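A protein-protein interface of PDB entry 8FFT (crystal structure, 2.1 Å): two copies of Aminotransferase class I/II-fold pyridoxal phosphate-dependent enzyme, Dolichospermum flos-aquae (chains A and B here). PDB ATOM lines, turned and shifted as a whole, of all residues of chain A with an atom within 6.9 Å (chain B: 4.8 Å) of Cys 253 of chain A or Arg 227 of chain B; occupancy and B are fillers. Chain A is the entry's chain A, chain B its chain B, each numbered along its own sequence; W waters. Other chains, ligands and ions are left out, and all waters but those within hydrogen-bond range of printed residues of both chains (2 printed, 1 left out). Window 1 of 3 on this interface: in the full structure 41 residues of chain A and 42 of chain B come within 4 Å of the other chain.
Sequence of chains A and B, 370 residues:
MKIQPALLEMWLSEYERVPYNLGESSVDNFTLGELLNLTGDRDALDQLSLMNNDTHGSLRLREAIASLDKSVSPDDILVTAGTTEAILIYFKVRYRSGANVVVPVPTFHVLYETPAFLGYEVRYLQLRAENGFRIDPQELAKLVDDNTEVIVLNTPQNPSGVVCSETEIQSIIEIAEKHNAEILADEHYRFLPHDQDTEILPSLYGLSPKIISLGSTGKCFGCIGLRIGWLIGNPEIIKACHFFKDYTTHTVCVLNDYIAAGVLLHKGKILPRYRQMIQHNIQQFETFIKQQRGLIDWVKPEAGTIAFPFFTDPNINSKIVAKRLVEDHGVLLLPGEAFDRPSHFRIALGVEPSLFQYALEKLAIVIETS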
ATOM      1  N   SER A  49     -13.519 -10.120   9.136  1.00  0.00           N
ATOM      2  CA  SER A  49     -13.028  -8.999   9.923  1.00  0.00           C
ATOM      3  C   SER A  49     -12.729  -9.425  11.354  1.00  0.00           C
ATOM      4  O   SER A  49     -13.490 -10.177  11.963  1.00  0.00           O
ATOM      5  CB  SER A  49     -14.054  -7.863   9.930  1.00  0.00           C
ATOM      6  OG  SER A  49     -13.660  -6.847  10.834  1.00  0.00           O
ATOM      7  N   LEU A  50     -11.621  -8.924  11.900  1.00  0.00           N
ATOM      8  CA  LEU A  50     -11.266  -9.197  13.285  1.00  0.00           C
ATOM      9  C   LEU A  50     -11.844  -8.167  14.248  1.00  0.00           C
ATOM     10  O   LEU A  50     -11.388  -8.076  15.396  1.00  0.00           O
ATOM     11  CB  LEU A  50      -9.747  -9.280  13.442  1.00  0.00           C
ATOM     12  CG  LEU A  50      -9.124 -10.427  12.649  1.00  0.00           C
ATOM     13  CD1 LEU A  50      -7.625 -10.472  12.843  1.00  0.00           C
ATOM     14  CD2 LEU A  50      -9.779 -11.774  13.000  1.00  0.00           C
ATOM     15  N   MET A  51     -12.822  -7.380  13.799  1.00  0.00           N
ATOM     16  CA  MET A  51     -13.632  -6.612  14.723  1.00  0.00           C
ATOM     17  C   MET A  51     -14.448  -7.572  15.586  1.00  0.00           C
ATOM     18  O   MET A  51     -14.496  -8.784  15.344  1.00  0.00           O
ATOM     19  CB  MET A  51     -14.562  -5.658  13.973  1.00  0.00           C
ATOM     20  CG  MET A  51     -15.692  -6.377  13.235  1.00  0.00           C
ATOM     21  SD  MET A  51     -16.786  -5.282  12.310  1.00  0.00           S
ATOM     22  CE  MET A  51     -15.591  -4.274  11.440  1.00  0.00           C
ATOM     23  N   ASN A  52     -15.111  -7.021  16.595  1.00  0.00           N
ATOM     24  CA  ASN A  52     -15.921  -7.853  17.475  1.00  0.00           C
ATOM     25  C   ASN A  52     -17.004  -8.562  16.669  1.00  0.00           C
ATOM     26  O   ASN A  52     -17.669  -7.956  15.826  1.00  0.00           O
ATOM     27  CB  ASN A  52     -16.550  -7.000  18.576  1.00  0.00           C
ATOM     28  CG  ASN A  52     -15.613  -6.782  19.757  1.00  0.00           C
ATOM     29  OD1 ASN A  52     -14.802  -7.647  20.093  1.00  0.00           O
ATOM     30  ND2 ASN A  52     -15.724  -5.619  20.388  1.00  0.00           N
ATOM     31  N   ASN A  53     -17.163  -9.855  16.920  1.00  0.00           N
ATOM     32  CA  ASN A  53     -18.228 -10.632  16.304  1.00  0.00           C
ATOM     33  C   ASN A  53     -19.588 -10.096  16.744  1.00  0.00           C
ATOM     34  O   ASN A  53     -19.700  -9.320  17.694  1.00  0.00           O
ATOM     35  CB  ASN A  53     -18.074 -12.101  16.697  1.00  0.00           C
ATOM     36  CG  ASN A  53     -18.994 -13.037  15.926  1.00  0.00           C
ATOM     37  OD1 ASN A  53     -19.514 -12.699  14.862  1.00  0.00           O
ATOM     38  ND2 ASN A  53     -19.182 -14.238  16.465  1.00  0.00           N
ATOM     39  N   ARG A 227     -13.838 -24.023  20.833  1.00  0.00           N
ATOM     40  CA  ARG A 227     -14.526 -23.352  21.938  1.00  0.00           C
ATOM     41  C   ARG A 227     -15.791 -22.643  21.444  1.00  0.00           C
ATOM     42  O   ARG A 227     -15.968 -21.434  21.595  1.00  0.00           O
ATOM     43  CB  ARG A 227     -13.598 -22.370  22.661  1.00  0.00           C
ATOM     44  CG  ARG A 227     -12.220 -22.928  22.993  1.00  0.00           C
ATOM     45  CD  ARG A 227     -12.285 -24.234  23.765  1.00  0.00           C
ATOM     46  NE  ARG A 227     -13.035 -24.098  25.008  1.00  0.00           N
ATOM     47  CZ  ARG A 227     -14.030 -24.895  25.375  1.00  0.00           C
ATOM     48  NH1 ARG A 227     -14.392 -25.918  24.601  1.00  0.00           N
ATOM     49  NH2 ARG A 227     -14.652 -24.681  26.526  1.00  0.00           N
ATOM     50  N   ILE A 228     -16.675 -23.423  20.836  1.00  0.00           N
ATOM     51  CA  ILE A 228     -17.958 -22.919  20.377  1.00  0.00           C
ATOM     52  C   ILE A 228     -19.051 -23.746  21.030  1.00  0.00           C
ATOM     53  O   ILE A 228     -19.090 -24.971  20.867  1.00  0.00           O
ATOM     54  CB  ILE A 228     -18.084 -22.955  18.846  1.00  0.00           C
ATOM     55  CG1 ILE A 228     -17.152 -21.921  18.212  1.00  0.00           C
ATOM     56  CG2 ILE A 228     -19.533 -22.704  18.432  1.00  0.00           C
ATOM     57  CD1 ILE A 228     -17.467 -20.494  18.610  1.00  0.00           C
ATOM     58  N   THR A 248     -18.128 -11.959  31.025  1.00  0.00           N
ATOM     59  CA  THR A 248     -17.349 -13.189  30.979  1.00  0.00           C
ATOM     60  C   THR A 248     -16.344 -13.121  29.836  1.00  0.00           C
ATOM     61  O   THR A 248     -15.142 -13.049  30.085  1.00  0.00           O
ATOM     62  CB  THR A 248     -18.271 -14.407  30.864  1.00  0.00           C
ATOM     63  OG1 THR A 248     -19.065 -14.307  29.676  1.00  0.00           O
ATOM     64  CG2 THR A 248     -19.205 -14.462  32.073  1.00  0.00           C
ATOM     65  N   THR A 249     -16.801 -13.110  28.582  1.00  0.00           N
ATOM     66  CA  THR A 249     -15.905 -13.031  27.436  1.00  0.00           C
ATOM     67  C   THR A 249     -16.346 -12.027  26.382  1.00  0.00           C
ATOM     68  O   THR A 249     -15.685 -11.925  25.341  1.00  0.00           O
ATOM     69  CB  THR A 249     -15.758 -14.398  26.754  1.00  0.00           C
ATOM     70  OG1 THR A 249     -17.031 -14.806  26.246  1.00  0.00           O
ATOM     71  CG2 THR A 249     -15.248 -15.451  27.736  1.00  0.00           C
ATOM     72  N   HIS A 250     -17.460 -11.326  26.593  1.00  0.00           N
ATOM     73  CA  HIS A 250     -18.011 -10.369  25.635  1.00  0.00           C
ATOM     74  C   HIS A 250     -18.449 -11.050  24.342  1.00  0.00           C
ATOM     75  O   HIS A 250     -19.652 -11.178  24.097  1.00  0.00           O
ATOM     76  CB  HIS A 250     -17.022  -9.235  25.335  1.00  0.00           C
ATOM     77  CG  HIS A 250     -17.602  -8.161  24.470  1.00  0.00           C
ATOM     78  ND1 HIS A 250     -16.873  -7.500  23.505  1.00  0.00           N
ATOM     79  CD2 HIS A 250     -18.855  -7.651  24.410  1.00  0.00           C
ATOM     80  CE1 HIS A 250     -17.649  -6.619  22.897  1.00  0.00           C
ATOM     81  NE2 HIS A 250     -18.857  -6.691  23.427  1.00  0.00           N
ATOM     82  N   THR A 251     -17.508 -11.453  23.487  1.00  0.00           N
ATOM     83  CA  THR A 251     -17.859 -12.140  22.248  1.00  0.00           C
ATOM     84  C   THR A 251     -16.910 -13.311  22.022  1.00  0.00           C
ATOM     85  O   THR A 251     -15.797 -13.347  22.561  1.00  0.00           O
ATOM     86  CB  THR A 251     -17.795 -11.228  21.008  1.00  0.00           C
ATOM     87  OG1 THR A 251     -16.445 -10.804  20.792  1.00  0.00           O
ATOM     88  CG2 THR A 251     -18.688 -10.008  21.164  1.00  0.00           C
ATOM     89  N   VAL A 252     -17.357 -14.265  21.190  1.00  0.00           N
ATOM     90  CA  VAL A 252     -16.486 -15.312  20.670  1.00  0.00           C
ATOM     91  C   VAL A 252     -15.908 -14.839  19.342  1.00  0.00           C
ATOM     92  O   VAL A 252     -16.508 -14.018  18.636  1.00  0.00           O
ATOM     93  CB  VAL A 252     -17.229 -16.663  20.538  1.00  0.00           C
ATOM     94  CG1 VAL A 252     -18.175 -16.870  21.709  1.00  0.00           C
ATOM     95  CG2 VAL A 252     -18.033 -16.708  19.245  1.00  0.00           C
ATOM     96  N   CYS A 253     -14.723 -15.347  19.003  1.00  0.00           N
ATOM     97  CA  CYS A 253     -14.037 -14.893  17.800  1.00  0.00           C
ATOM     98  C   CYS A 253     -14.836 -15.219  16.545  1.00  0.00           C
ATOM     99  O   CYS A 253     -15.477 -16.269  16.449  1.00  0.00           O
ATOM    100  CB  CYS A 253     -12.651 -15.529  17.692  1.00  0.00           C
ATOM    101  SG  CYS A 253     -11.765 -15.032  16.179  1.00  0.00           S
ATOM    102  N   VAL A 254     -14.788 -14.302  15.576  1.00  0.00           N
ATOM    103  CA  VAL A 254     -15.470 -14.523  14.304  1.00  0.00           C
ATOM    104  C   VAL A 254     -14.893 -15.741  13.598  1.00  0.00           C
ATOM    105  O   VAL A 254     -15.601 -16.444  12.865  1.00  0.00           O
ATOM    106  CB  VAL A 254     -15.377 -13.255  13.427  1.00  0.00           C
ATOM    107  CG1 VAL A 254     -13.923 -12.939  13.092  1.00  0.00           C
ATOM    108  CG2 VAL A 254     -16.205 -13.400  12.162  1.00  0.00           C
ATOM    109  N   LEU A 255     -13.608 -16.023  13.822  1.00  0.00           N
ATOM    110  CA  LEU A 255     -12.952 -17.140  13.151  1.00  0.00           C
ATOM    111  C   LEU A 255     -13.500 -18.479  13.634  1.00  0.00           C
ATOM    112  O   LEU A 255     -13.920 -19.314  12.826  1.00  0.00           O
ATOM    113  CB  LEU A 255     -11.444 -17.039  13.373  1.00  0.00           C
ATOM    114  CG  LEU A 255     -10.484 -18.132  12.919  1.00  0.00           C
ATOM    115  CD1 LEU A 255     -10.688 -18.465  11.448  1.00  0.00           C
ATOM    116  CD2 LEU A 255      -9.046 -17.660  13.181  1.00  0.00           C
ATOM    117  N   ASN A 256     -13.512 -18.702  14.952  1.00  0.00           N
ATOM    118  CA  ASN A 256     -14.075 -19.940  15.492  1.00  0.00           C
ATOM    119  C   ASN A 256     -15.553 -20.064  15.156  1.00  0.00           C
ATOM    120  O   ASN A 256     -16.032 -21.144  14.783  1.00  0.00           O
ATOM    121  CB  ASN A 256     -13.896 -19.975  17.005  1.00  0.00           C
ATOM    122  CG  ASN A 256     -12.462 -19.802  17.420  1.00  0.00           C
ATOM    123  OD1 ASN A 256     -12.038 -18.701  17.745  1.00  0.00           O
ATOM    124  ND2 ASN A 256     -11.705 -20.889  17.420  1.00  0.00           N
ATOM    125  N   ASP A 257     -16.291 -18.967  15.316  1.00  0.00           N
ATOM    126  CA  ASP A 257     -17.691 -18.898  14.919  1.00  0.00           C
ATOM    127  C   ASP A 257     -17.875 -19.385  13.487  1.00  0.00           C
ATOM    128  O   ASP A 257     -18.706 -20.263  13.212  1.00  0.00           O
ATOM    129  CB  ASP A 257     -18.168 -17.451  15.094  1.00  0.00           C
ATOM    130  CG  ASP A 257     -19.633 -17.253  14.779  1.00  0.00           C
ATOM    131  OD1 ASP A 257     -20.112 -17.741  13.728  1.00  0.00           O
ATOM    132  OD2 ASP A 257     -20.307 -16.578  15.586  1.00  0.00           O
ATOM    133  N   TYR A 258     -17.093 -18.830  12.563  1.00  0.00           N
ATOM    134  CA  TYR A 258     -17.248 -19.171  11.155  1.00  0.00           C
ATOM    135  C   TYR A 258     -16.902 -20.633  10.896  1.00  0.00           C
ATOM    136  O   TYR A 258     -17.596 -21.316  10.131  1.00  0.00           O
ATOM    137  CB  TYR A 258     -16.382 -18.251  10.308  1.00  0.00           C
ATOM    138  CG  TYR A 258     -16.775 -18.198   8.861  1.00  0.00           C
ATOM    139  CD1 TYR A 258     -17.710 -17.274   8.409  1.00  0.00           C
ATOM    140  CD2 TYR A 258     -16.203 -19.059   7.939  1.00  0.00           C
ATOM    141  CE1 TYR A 258     -18.065 -17.215   7.071  1.00  0.00           C
ATOM    142  CE2 TYR A 258     -16.552 -19.007   6.606  1.00  0.00           C
ATOM    143  CZ  TYR A 258     -17.482 -18.088   6.179  1.00  0.00           C
ATOM    144  OH  TYR A 258     -17.822 -18.051   4.852  1.00  0.00           O
ATOM    145  N   THR B  80      -6.189 -15.823  28.708  1.00  0.00           N
ATOM    146  CA  THR B  80      -7.638 -15.888  28.843  1.00  0.00           C
ATOM    147  C   THR B  80      -8.287 -15.362  27.572  1.00  0.00           C
ATOM    148  O   THR B  80      -7.625 -14.790  26.698  1.00  0.00           O
ATOM    149  CB  THR B  80      -8.161 -15.084  30.047  1.00  0.00           C
ATOM    150  OG1 THR B  80      -7.749 -13.714  29.935  1.00  0.00           O
ATOM    151  CG2 THR B  80      -7.677 -15.683  31.366  1.00  0.00           C
ATOM    152  N   ALA B  81      -9.604 -15.563  27.485  1.00  0.00           N
ATOM    153  CA  ALA B  81     -10.401 -15.100  26.351  1.00  0.00           C
ATOM    154  C   ALA B  81     -10.740 -13.630  26.574  1.00  0.00           C
ATOM    155  O   ALA B  81     -11.842 -13.260  26.993  1.00  0.00           O
ATOM    156  CB  ALA B  81     -11.658 -15.946  26.192  1.00  0.00           C
ATOM    157  N   GLY B  82      -9.769 -12.777  26.273  1.00  0.00           N
ATOM    158  CA  GLY B  82      -9.849 -11.370  26.596  1.00  0.00           C
ATOM    159  C   GLY B  82      -9.540 -11.102  28.060  1.00  0.00           C
ATOM    160  O   GLY B  82      -9.546 -11.994  28.909  1.00  0.00           O
ATOM    161  N   THR B  84     -11.475  -9.409  29.849  1.00  0.00           N
ATOM    162  CA  THR B  84     -12.755  -9.499  30.540  1.00  0.00           C
ATOM    163  C   THR B  84     -12.855 -10.795  31.334  1.00  0.00           C
ATOM    164  O   THR B  84     -13.295 -10.790  32.490  1.00  0.00           O
ATOM    165  CB  THR B  84     -13.899  -9.386  29.528  1.00  0.00           C
ATOM    166  OG1 THR B  84     -13.858  -8.093  28.908  1.00  0.00           O
ATOM    167  CG2 THR B  84     -15.243  -9.569  30.211  1.00  0.00           C
ATOM    168  N1  LLP B 219     -10.144  -2.987  30.103  1.00  0.00           N
ATOM    169  C2  LLP B 219      -9.869  -1.944  29.314  1.00  0.00           C
ATOM    170  C2' LLP B 219      -9.253  -0.736  29.951  1.00  0.00           C
ATOM    171  C3  LLP B 219     -10.144  -1.971  27.940  1.00  0.00           C
ATOM    172  O3  LLP B 219      -9.834  -0.870  27.217  1.00  0.00           O
ATOM    173  C4  LLP B 219     -10.720  -3.121  27.374  1.00  0.00           C
ATOM    174  C4' LLP B 219     -11.018  -3.173  25.942  1.00  0.00           C
ATOM    175  C5  LLP B 219     -11.001  -4.215  28.222  1.00  0.00           C
ATOM    176  C6  LLP B 219     -10.688  -4.078  29.556  1.00  0.00           C
ATOM    177  C5' LLP B 219     -11.639  -5.491  27.739  1.00  0.00           C
ATOM    178  OP4 LLP B 219     -11.306  -5.904  26.401  1.00  0.00           O
ATOM    179  P   LLP B 219     -11.074  -7.470  26.141  1.00  0.00           P
ATOM    180  OP1 LLP B 219     -12.000  -8.273  26.986  1.00  0.00           O
ATOM    181  OP2 LLP B 219      -9.599  -7.708  26.465  1.00  0.00           O
ATOM    182  OP3 LLP B 219     -11.293  -7.679  24.640  1.00  0.00           O
ATOM    183  N   LLP B 219      -6.876  -4.379  21.589  1.00  0.00           N
ATOM    184  CA  LLP B 219      -7.175  -2.958  21.342  1.00  0.00           C
ATOM    185  CB  LLP B 219      -7.373  -2.233  22.676  1.00  0.00           C
ATOM    186  CG  LLP B 219      -8.623  -2.706  23.421  1.00  0.00           C
ATOM    187  CD  LLP B 219      -9.935  -2.224  22.822  1.00  0.00           C
ATOM    188  CE  LLP B 219     -11.140  -2.497  23.711  1.00  0.00           C
ATOM    189  NZ  LLP B 219     -10.801  -2.243  25.107  1.00  0.00           N
ATOM    190  C   LLP B 219      -6.097  -2.262  20.523  1.00  0.00           C
ATOM    191  O   LLP B 219      -6.371  -1.322  19.815  1.00  0.00           O
ATOM    192  N   CYS B 223      -7.021  -6.457  16.212  1.00  0.00           N
ATOM    193  CA  CYS B 223      -7.581  -7.806  16.221  1.00  0.00           C
ATOM    194  C   CYS B 223      -8.331  -8.047  17.525  1.00  0.00           C
ATOM    195  O   CYS B 223      -8.137  -9.053  18.209  1.00  0.00           O
ATOM    196  CB  CYS B 223      -6.477  -8.837  16.021  1.00  0.00           C
ATOM    197  SG  CYS B 223      -5.147  -8.634  17.213  1.00  0.00           S
ATOM    198  N   ILE B 224      -9.210  -7.107  17.878  1.00  0.00           N
ATOM    199  CA  ILE B 224      -9.969  -7.211  19.119  1.00  0.00           C
ATOM    200  C   ILE B 224     -10.814  -8.482  19.115  1.00  0.00           C
ATOM    201  O   ILE B 224     -11.059  -9.077  20.168  1.00  0.00           O
ATOM    202  CB  ILE B 224     -10.823  -5.937  19.319  1.00  0.00           C
ATOM    203  CG1 ILE B 224     -11.499  -5.920  20.694  1.00  0.00           C
ATOM    204  CG2 ILE B 224     -11.862  -5.794  18.212  1.00  0.00           C
ATOM    205  CD1 ILE B 224     -10.524  -5.896  21.857  1.00  0.00           C
ATOM    206  N   GLY B 225     -11.246  -8.930  17.937  1.00  0.00           N
ATOM    207  CA  GLY B 225     -12.093 -10.104  17.827  1.00  0.00           C
ATOM    208  C   GLY B 225     -11.405 -11.425  18.122  1.00  0.00           C
ATOM    209  O   GLY B 225     -12.102 -12.426  18.303  1.00  0.00           O
ATOM    210  N   LEU B 226     -10.070 -11.462  18.179  1.00  0.00           N
ATOM    211  CA  LEU B 226      -9.398 -12.723  18.488  1.00  0.00           C
ATOM    212  C   LEU B 226      -9.718 -13.213  19.895  1.00  0.00           C
ATOM    213  O   LEU B 226      -9.690 -14.423  20.143  1.00  0.00           O
ATOM    214  CB  LEU B 226      -7.887 -12.586  18.325  1.00  0.00           C
ATOM    215  CG  LEU B 226      -7.367 -12.573  16.892  1.00  0.00           C
ATOM    216  CD1 LEU B 226      -5.847 -12.483  16.907  1.00  0.00           C
ATOM    217  CD2 LEU B 226      -7.844 -13.815  16.132  1.00  0.00           C
ATOM    218  N   ARG B 227     -10.033 -12.297  20.815  1.00  0.00           N
ATOM    219  CA  ARG B 227     -10.351 -12.625  22.208  1.00  0.00           C
ATOM    220  C   ARG B 227      -9.166 -13.313  22.892  1.00  0.00           C
ATOM    221  O   ARG B 227      -9.260 -14.430  23.399  1.00  0.00           O
ATOM    222  CB  ARG B 227     -11.618 -13.485  22.299  1.00  0.00           C
ATOM    223  CG  ARG B 227     -12.795 -12.979  21.466  1.00  0.00           C
ATOM    224  CD  ARG B 227     -13.158 -11.530  21.769  1.00  0.00           C
ATOM    225  NE  ARG B 227     -13.485 -11.340  23.176  1.00  0.00           N
ATOM    226  CZ  ARG B 227     -12.943 -10.416  23.960  1.00  0.00           C
ATOM    227  NH1 ARG B 227     -12.047  -9.557  23.479  1.00  0.00           N
ATOM    228  NH2 ARG B 227     -13.320 -10.337  25.230  1.00  0.00           N
ATOM    229  N   ILE B 228      -8.034 -12.620  22.898  1.00  0.00           N
ATOM    230  CA  ILE B 228      -6.837 -13.089  23.582  1.00  0.00           C
ATOM    231  C   ILE B 228      -6.434 -12.031  24.591  1.00  0.00           C
ATOM    232  O   ILE B 228      -6.137 -10.890  24.220  1.00  0.00           O
ATOM    233  CB  ILE B 228      -5.686 -13.384  22.611  1.00  0.00           C
ATOM    234  CG1 ILE B 228      -5.999 -14.630  21.785  1.00  0.00           C
ATOM    235  CG2 ILE B 228      -4.371 -13.548  23.376  1.00  0.00           C
ATOM    236  CD1 ILE B 228      -6.141 -15.887  22.620  1.00  0.00           C
ATOM    237  N   GLY B 229      -6.433 -12.409  25.867  1.00  0.00           N
ATOM    238  CA  GLY B 229      -5.869 -11.587  26.915  1.00  0.00           C
ATOM    239  C   GLY B 229      -4.995 -12.437  27.818  1.00  0.00           C
ATOM    240  O   GLY B 229      -4.841 -13.641  27.609  1.00  0.00           O
ATOM    241  N   ASN B 256      -6.651 -18.907  17.837  1.00  0.00           N
ATOM    242  CA  ASN B 256      -6.501 -17.541  18.338  1.00  0.00           C
ATOM    243  C   ASN B 256      -5.196 -17.377  19.094  1.00  0.00           C
ATOM    244  O   ASN B 256      -4.498 -16.364  18.942  1.00  0.00           O
ATOM    245  CB  ASN B 256      -7.657 -17.195  19.270  1.00  0.00           C
ATOM    246  CG  ASN B 256      -8.989 -17.397  18.629  1.00  0.00           C
ATOM    247  OD1 ASN B 256      -9.379 -18.523  18.346  1.00  0.00           O
ATOM    248  ND2 ASN B 256      -9.709 -16.312  18.406  1.00  0.00           N
HETATM  249  O   HOH W   1     -14.215 -11.612  15.951  1.00  0.00           O
HETATM  250  O   HOH W   2     -15.415 -11.570  18.435  1.00  0.00           O
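Hydrophobic or aromatic side chains of chain A within 4 Å of the printed part of chain B: Leu 50 and His 250.
Hydrophobic or aromatic side chains of chain B within 4 Å of the printed part of chain A: Ala 81 and Ile 224.
Among the printed residues, no Asp or Glu carboxylate lies within 4 Å of a Lys or Arg side-chain nitrogen of the other chain.
Asn 256 of chain A touches its own counterpart, Asn 256 of chain B.
Of the 16 pairs that touch across the chains among the printed residues, 1 has its exchanged pair printed and touching as well.
Ile 228 of chain A touches none of the printed residues of chain B.
Of the printed residues of chain B, Cys 253 of chain A touches Gly 225, Leu 226, Arg 227 and Asn 256.
Printed residues of chain B within 4 Å of Asn 256 of chain A: Asn 256.
Of the printed residues of chain A, Ala 81 of chain B touches Thr 249.
Of the printed residues of chain A, Leu 226 of chain B touches Cys 253 (3.9998 Å).
Arg 227 of chain B touches four residues of chain A.
The nearest printed residue of chain B that does not touch Cys 253 of chain A is Ile 224 of chain B (6.9 Å).
The nearest residue of chain A that does not touch Arg 227 of chain B is Val 252 of chain A (4.2 Å).
The nearest printed residue of chain B that does not touch Thr 251 of chain A is Gly 225 of chain B (5.3 Å).
Water W2 lies within hydrogen-bond range of the side-chain hydroxyl of Thr 251 of chain A (2.7 Å), the backbone carbonyl oxygen of Val 252 of chain A (2.7 Å), the backbone NH of Asn 53 of chain A (2.9 Å) and the backbone carbonyl oxygen of Gly 225 of chain B (3.4 Å).
Water W1 lies within hydrogen-bond range of N of Val 254 of chain A (2.8 Å), O of Met 51 of chain A (2.9 Å) and O of Gly 225 of chain B (3.3 Å).
The backbone NH of Met 51 of chain A lies within hydrogen-bond range of the side-chain hydroxyl of Ser 49 of chain A (3.1 Å).
SG of Cys 253 of chain A sits close to N of Leu 255 of chain A.
The backbone carbonyl oxygen (O) of Arg 227 of chain B lies within hydrogen-bond range of the backbone NH (N) of Gly 82 of chain B (3.4 Å).
OP1 of LLP 219 of chain B is in hydrogen-bond range of the side-chain hydroxyl (OG1) of Thr 84 of chain B (2.7 Å).
OP1 of LLP 219 of chain B lies close to NH2 of Arg 227 of chain B (3.0 Å).
The side-chain amide nitrogen of Asn 256 of chain B sits at hydrogen-bond distance from the backbone carbonyl oxygen of Leu 226 of chain B (2.6 Å).
Among the printed residues, pairs that only touch across the chains: Thr 248 of chain A with Thr 84 of chain B (3.4 Å), Met 51 of chain A with Gly 225 of chain B (3.7 Å), Leu 50 of chain A with Cys 223 of chain B (3.7 Å), Asn 52 of chain A with Ile 224 of chain B (3.8 Å), His 250 of chain A with Arg 227 of chain B (3.9 Å), Cys 253 of chain A with Arg 227 of chain B (3.9 Å), Thr 249 of chain A with Ala 81 of chain B (3.9 Å), Met 51 of chain A with Ile 224 of chain B (3.997 Å) and Cys 253 of chain A with Leu 226 of chain B (3.9998 Å).
O of Leu 50 of chain A lies within hydrogen-bond range of N of Ile 224 of chain B (3.4 Å).
The backbone NH of Gly 225 of chain B sits at hydrogen-bond distance from the backbone carbonyl oxygen of Leu 50 of chain A (2.7 Å).
The backbone carbonyl oxygen of Thr 249 of chain A lies within hydrogen-bond range of the guanidinium group of Arg 227 of chain B (2.9 Å).
The guanidinium group of Arg 227 of chain B sits at hydrogen-bond distance from the backbone carbonyl oxygen of Thr 251 of chain A (3.1 Å).
O of Gly 225 of chain B lies close to SG of Cys 253 of chain A (3.4 Å).
The side-chain sulfur of Cys 253 of chain A sits close to the side-chain amide nitrogen of Asn 256 of chain B (3.3 Å).
OD1 of Asn 256 of chain A sits close to OD1 of Asn 256 of chain B (2.7 Å).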
